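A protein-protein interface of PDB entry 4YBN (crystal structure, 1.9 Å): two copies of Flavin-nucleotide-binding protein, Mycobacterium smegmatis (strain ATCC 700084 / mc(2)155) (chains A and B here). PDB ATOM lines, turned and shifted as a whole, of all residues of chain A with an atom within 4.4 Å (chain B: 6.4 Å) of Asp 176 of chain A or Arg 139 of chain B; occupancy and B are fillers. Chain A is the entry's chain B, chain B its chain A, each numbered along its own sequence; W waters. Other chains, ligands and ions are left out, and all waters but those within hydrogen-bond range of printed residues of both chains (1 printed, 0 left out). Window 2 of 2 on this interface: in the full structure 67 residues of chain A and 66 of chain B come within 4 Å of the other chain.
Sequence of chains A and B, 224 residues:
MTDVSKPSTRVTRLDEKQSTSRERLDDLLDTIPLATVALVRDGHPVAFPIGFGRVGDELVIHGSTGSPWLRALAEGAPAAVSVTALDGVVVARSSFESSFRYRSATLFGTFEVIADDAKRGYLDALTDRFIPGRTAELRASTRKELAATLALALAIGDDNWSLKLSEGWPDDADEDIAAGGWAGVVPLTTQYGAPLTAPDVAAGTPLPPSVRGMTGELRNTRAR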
ATOM      1  N   ARG A  93      17.666  13.589  27.094  1.00  0.00           N
ATOM      2  CA  ARG A  93      16.562  13.839  28.048  1.00  0.00           C
ATOM      3  C   ARG A  93      15.311  13.079  27.676  1.00  0.00           C
ATOM      4  O   ARG A  93      14.445  12.876  28.553  1.00  0.00           O
ATOM      5  CB  ARG A  93      16.266  15.354  28.168  1.00  0.00           C
ATOM      6  CG  ARG A  93      17.356  16.091  28.893  1.00  0.00           C
ATOM      7  CD  ARG A  93      17.120  17.594  28.860  1.00  0.00           C
ATOM      8  NE  ARG A  93      18.291  18.402  29.279  1.00  0.00           N
ATOM      9  CZ  ARG A  93      19.395  18.616  28.534  1.00  0.00           C
ATOM     10  NH1 ARG A  93      19.555  18.066  27.328  1.00  0.00           N
ATOM     11  NH2 ARG A  93      20.378  19.385  29.019  1.00  0.00           N
ATOM     12  N   SER A  94      15.232  12.612  26.419  1.00  0.00           N
ATOM     13  CA  SER A  94      14.119  11.838  25.917  1.00  0.00           C
ATOM     14  C   SER A  94      14.672  10.557  25.330  1.00  0.00           C
ATOM     15  O   SER A  94      15.811  10.496  24.834  1.00  0.00           O
ATOM     16  CB  SER A  94      13.388  12.575  24.772  1.00  0.00           C
ATOM     17  OG  SER A  94      14.161  12.643  23.568  1.00  0.00           O
ATOM     18  N   ALA A 173      14.958  18.729  22.628  1.00  0.00           N
ATOM     19  CA  ALA A 173      14.012  19.868  22.502  1.00  0.00           C
ATOM     20  C   ALA A 173      14.165  20.828  23.667  1.00  0.00           C
ATOM     21  O   ALA A 173      14.513  20.415  24.790  1.00  0.00           O
ATOM     22  CB  ALA A 173      12.598  19.347  22.499  1.00  0.00           C
ATOM     23  N   ASP A 174      13.811  22.077  23.395  1.00  0.00           N
ATOM     24  CA  ASP A 174      13.915  23.182  24.348  1.00  0.00           C
ATOM     25  C   ASP A 174      13.169  22.921  25.644  1.00  0.00           C
ATOM     26  O   ASP A 174      13.647  23.235  26.726  1.00  0.00           O
ATOM     27  CB  ASP A 174      13.402  24.448  23.645  1.00  0.00           C
ATOM     28  CG  ASP A 174      14.220  24.769  22.414  1.00  0.00           C
ATOM     29  OD1 ASP A 174      15.227  24.082  22.239  1.00  0.00           O
ATOM     30  OD2 ASP A 174      13.875  25.671  21.626  1.00  0.00           O
ATOM     31  N   GLU A 175      12.011  22.290  25.501  1.00  0.00           N
ATOM     32  CA  GLU A 175      11.103  21.960  26.605  1.00  0.00           C
ATOM     33  C   GLU A 175      11.708  20.953  27.571  1.00  0.00           C
ATOM     34  O   GLU A 175      11.497  21.023  28.779  1.00  0.00           O
ATOM     35  CB  GLU A 175       9.803  21.341  26.073  1.00  0.00           C
ATOM     36  CG  GLU A 175       8.874  22.278  25.286  1.00  0.00           C
ATOM     37  CD  GLU A 175       9.473  22.827  23.982  1.00  0.00           C
ATOM     38  OE1 GLU A 175      10.554  22.345  23.532  1.00  0.00           O
ATOM     39  OE2 GLU A 175       8.849  23.756  23.402  1.00  0.00           O
ATOM     40  N   ASP A 176      12.458  20.006  27.025  1.00  0.00           N
ATOM     41  CA  ASP A 176      13.149  19.042  27.837  1.00  0.00           C
ATOM     42  C   ASP A 176      14.362  19.713  28.505  1.00  0.00           C
ATOM     43  O   ASP A 176      14.619  19.467  29.689  1.00  0.00           O
ATOM     44  CB  ASP A 176      13.592  17.832  27.020  1.00  0.00           C
ATOM     45  CG  ASP A 176      12.417  16.986  26.522  1.00  0.00           C
ATOM     46  OD1 ASP A 176      11.492  16.698  27.325  1.00  0.00           O
ATOM     47  OD2 ASP A 176      12.475  16.567  25.340  1.00  0.00           O
ATOM     48  N   ILE A 177      15.103  20.541  27.788  1.00  0.00           N
ATOM     49  CA  ILE A 177      16.256  21.226  28.462  1.00  0.00           C
ATOM     50  C   ILE A 177      15.706  22.033  29.646  1.00  0.00           C
ATOM     51  O   ILE A 177      16.173  21.915  30.728  1.00  0.00           O
ATOM     52  CB  ILE A 177      17.019  22.126  27.511  1.00  0.00           C
ATOM     53  CG1 ILE A 177      17.663  21.266  26.428  1.00  0.00           C
ATOM     54  CG2 ILE A 177      18.079  22.918  28.264  1.00  0.00           C
ATOM     55  CD1 ILE A 177      17.966  21.975  25.116  1.00  0.00           C
ATOM     56  N   ALA A 178      14.632  22.761  29.422  1.00  0.00           N
ATOM     57  CA  ALA A 178      14.035  23.598  30.441  1.00  0.00           C
ATOM     58  C   ALA A 178      13.460  22.840  31.599  1.00  0.00           C
ATOM     59  O   ALA A 178      13.391  23.374  32.696  1.00  0.00           O
ATOM     60  CB  ALA A 178      12.976  24.497  29.818  1.00  0.00           C
ATOM     61  N   ALA A 179      13.076  21.591  31.386  1.00  0.00           N
ATOM     62  CA  ALA A 179      12.652  20.725  32.458  1.00  0.00           C
ATOM     63  C   ALA A 179      13.804  20.174  33.290  1.00  0.00           C
ATOM     64  O   ALA A 179      13.579  19.618  34.380  1.00  0.00           O
ATOM     65  CB  ALA A 179      11.823  19.556  31.895  1.00  0.00           C
ATOM     66  N   GLY A 180      15.025  20.302  32.797  1.00  0.00           N
ATOM     67  CA  GLY A 180      16.173  19.865  33.571  1.00  0.00           C
ATOM     68  C   GLY A 180      16.564  18.459  33.150  1.00  0.00           C
ATOM     69  O   GLY A 180      16.310  18.062  32.023  1.00  0.00           O
ATOM     70  N   THR B 135      13.672   4.235  31.380  1.00  0.00           N
ATOM     71  CA  THR B 135      12.327   4.609  31.020  1.00  0.00           C
ATOM     72  C   THR B 135      11.628   5.225  32.231  1.00  0.00           C
ATOM     73  O   THR B 135      10.866   6.155  32.081  1.00  0.00           O
ATOM     74  CB  THR B 135      11.555   3.394  30.477  1.00  0.00           C
ATOM     75  OG1 THR B 135      12.018   3.110  29.145  1.00  0.00           O
ATOM     76  CG2 THR B 135      10.106   3.639  30.399  1.00  0.00           C
ATOM     77  N   ALA B 136      11.878   4.699  33.414  1.00  0.00           N
ATOM     78  CA  ALA B 136      11.155   5.183  34.573  1.00  0.00           C
ATOM     79  C   ALA B 136      11.614   6.596  34.880  1.00  0.00           C
ATOM     80  O   ALA B 136      10.907   7.316  35.538  1.00  0.00           O
ATOM     81  CB  ALA B 136      11.413   4.266  35.756  1.00  0.00           C
ATOM     82  N   GLU B 137      12.800   6.996  34.421  1.00  0.00           N
ATOM     83  CA  GLU B 137      13.310   8.375  34.654  1.00  0.00           C
ATOM     84  C   GLU B 137      12.876   9.434  33.647  1.00  0.00           C
ATOM     85  O   GLU B 137      13.042  10.603  33.884  1.00  0.00           O
ATOM     86  CB  GLU B 137      14.835   8.387  34.746  1.00  0.00           C
ATOM     87  CG  GLU B 137      15.427   7.445  35.839  1.00  0.00           C
ATOM     88  CD  GLU B 137      16.914   7.105  35.648  1.00  0.00           C
ATOM     89  OE1 GLU B 137      17.499   7.530  34.608  1.00  0.00           O
ATOM     90  OE2 GLU B 137      17.482   6.392  36.531  1.00  0.00           O
ATOM     91  N   LEU B 138      12.374   9.033  32.492  1.00  0.00           N
ATOM     92  CA  LEU B 138      12.074   9.964  31.447  1.00  0.00           C
ATOM     93  C   LEU B 138      10.551  10.190  31.334  1.00  0.00           C
ATOM     94  O   LEU B 138       9.751   9.327  31.647  1.00  0.00           O
ATOM     95  CB  LEU B 138      12.540   9.381  30.106  1.00  0.00           C
ATOM     96  CG  LEU B 138      13.970   8.942  29.910  1.00  0.00           C
ATOM     97  CD1 LEU B 138      14.094   7.963  28.773  1.00  0.00           C
ATOM     98  CD2 LEU B 138      14.804  10.141  29.574  1.00  0.00           C
ATOM     99  N   ARG B 139      10.181  11.329  30.810  1.00  0.00           N
ATOM    100  CA  ARG B 139       8.845  11.522  30.236  1.00  0.00           C
ATOM    101  C   ARG B 139       8.476  10.467  29.175  1.00  0.00           C
ATOM    102  O   ARG B 139       9.348   9.875  28.515  1.00  0.00           O
ATOM    103  CB  ARG B 139       8.704  12.891  29.583  1.00  0.00           C
ATOM    104  CG  ARG B 139       9.424  13.132  28.278  1.00  0.00           C
ATOM    105  CD  ARG B 139       8.967  14.421  27.624  1.00  0.00           C
ATOM    106  NE  ARG B 139       9.763  14.800  26.438  1.00  0.00           N
ATOM    107  CZ  ARG B 139       9.733  14.176  25.250  1.00  0.00           C
ATOM    108  NH1 ARG B 139       9.002  13.102  25.036  1.00  0.00           N
ATOM    109  NH2 ARG B 139      10.526  14.572  24.285  1.00  0.00           N
ATOM    110  N   ALA B 140       7.173  10.231  29.064  1.00  0.00           N
ATOM    111  CA  ALA B 140       6.579   9.418  28.006  1.00  0.00           C
ATOM    112  C   ALA B 140       6.935  10.045  26.676  1.00  0.00           C
ATOM    113  O   ALA B 140       6.964  11.260  26.531  1.00  0.00           O
ATOM    114  CB  ALA B 140       5.060   9.392  28.142  1.00  0.00           C
ATOM    115  N   SER B 141       7.102   9.209  25.667  1.00  0.00           N
ATOM    116  CA  SER B 141       7.304   9.706  24.321  1.00  0.00           C
ATOM    117  C   SER B 141       6.022  10.370  23.836  1.00  0.00           C
ATOM    118  O   SER B 141       4.927  10.005  24.285  1.00  0.00           O
ATOM    119  CB  SER B 141       7.676   8.522  23.430  1.00  0.00           C
ATOM    120  OG  SER B 141       8.968   8.006  23.815  1.00  0.00           O
ATOM    121  N   THR B 142       6.144  11.324  22.936  1.00  0.00           N
ATOM    122  CA  THR B 142       4.986  11.995  22.438  1.00  0.00           C
ATOM    123  C   THR B 142       4.434  11.275  21.259  1.00  0.00           C
ATOM    124  O   THR B 142       5.142  10.472  20.612  1.00  0.00           O
ATOM    125  CB  THR B 142       5.302  13.413  21.963  1.00  0.00           C
ATOM    126  OG1 THR B 142       6.195  13.364  20.870  1.00  0.00           O
ATOM    127  CG2 THR B 142       5.866  14.243  23.094  1.00  0.00           C
ATOM    128  N   GLU B 145       6.669  11.807  18.302  1.00  0.00           N
ATOM    129  CA  GLU B 145       7.862  10.976  18.381  1.00  0.00           C
ATOM    130  C   GLU B 145       7.553   9.539  17.940  1.00  0.00           C
ATOM    131  O   GLU B 145       8.317   8.934  17.170  1.00  0.00           O
ATOM    132  CB  GLU B 145       8.483  10.981  19.793  1.00  0.00           C
ATOM    133  CG  GLU B 145       9.163  12.314  20.128  1.00  0.00           C
ATOM    134  CD  GLU B 145       9.464  12.504  21.608  1.00  0.00           C
ATOM    135  OE1 GLU B 145       8.907  11.782  22.459  1.00  0.00           O
ATOM    136  OE2 GLU B 145      10.330  13.367  21.910  1.00  0.00           O
HETATM  137  O   HOH W   1      12.492  13.211  30.241  1.00  0.00           O
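No position is printed for both chains.
Among the printed residues, merely in contact across the chains: Arg 93 of chain A with Leu 138 of chain B and Ser 94 of chain A with Arg 139 of chain B.
The guanidinium group (NE) of Arg 139 of chain B lies within salt-bridge range of the side-chain carboxylate (OD1) of Asp 176 of chain A, at 2.7 Å.
Water W1 bridges the backbone carbonyl oxygen (O) of Arg 93 of chain A (2.6 Å) and the backbone NH (N) of Arg 139 of chain B (3.0 Å).
Of chain A, only Ser 94 and Asp 176 come within 4 Å of Arg 139 of chain B.
Of the printed residues of chain B, Ser 94 of chain A touches Arg 139.
Printed residues of chain B within 4 Å of Arg 93 of chain A: Leu 138.
Of the printed residues of chain A, Leu 138 of chain B touches Arg 93.
Ala 178 of chain A touches none of the printed residues of chain B.
Glu 137 of chain B touches none of the printed residues of chain A.
NH2 of Arg 139 of chain B lies within salt-bridge range of OE2 of Glu 145 of chain B.
The guanidinium group of Arg 93 of chain A sits close to the backbone carbonyl oxygen of Gly 180 of chain A (3.4 Å).
Printed residues of chain B that touch a printed residue of chain A: Leu 138 and Arg 139.
Hydrophobic or aromatic side chains of chain B that line the printed part of chain A: Leu 138.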
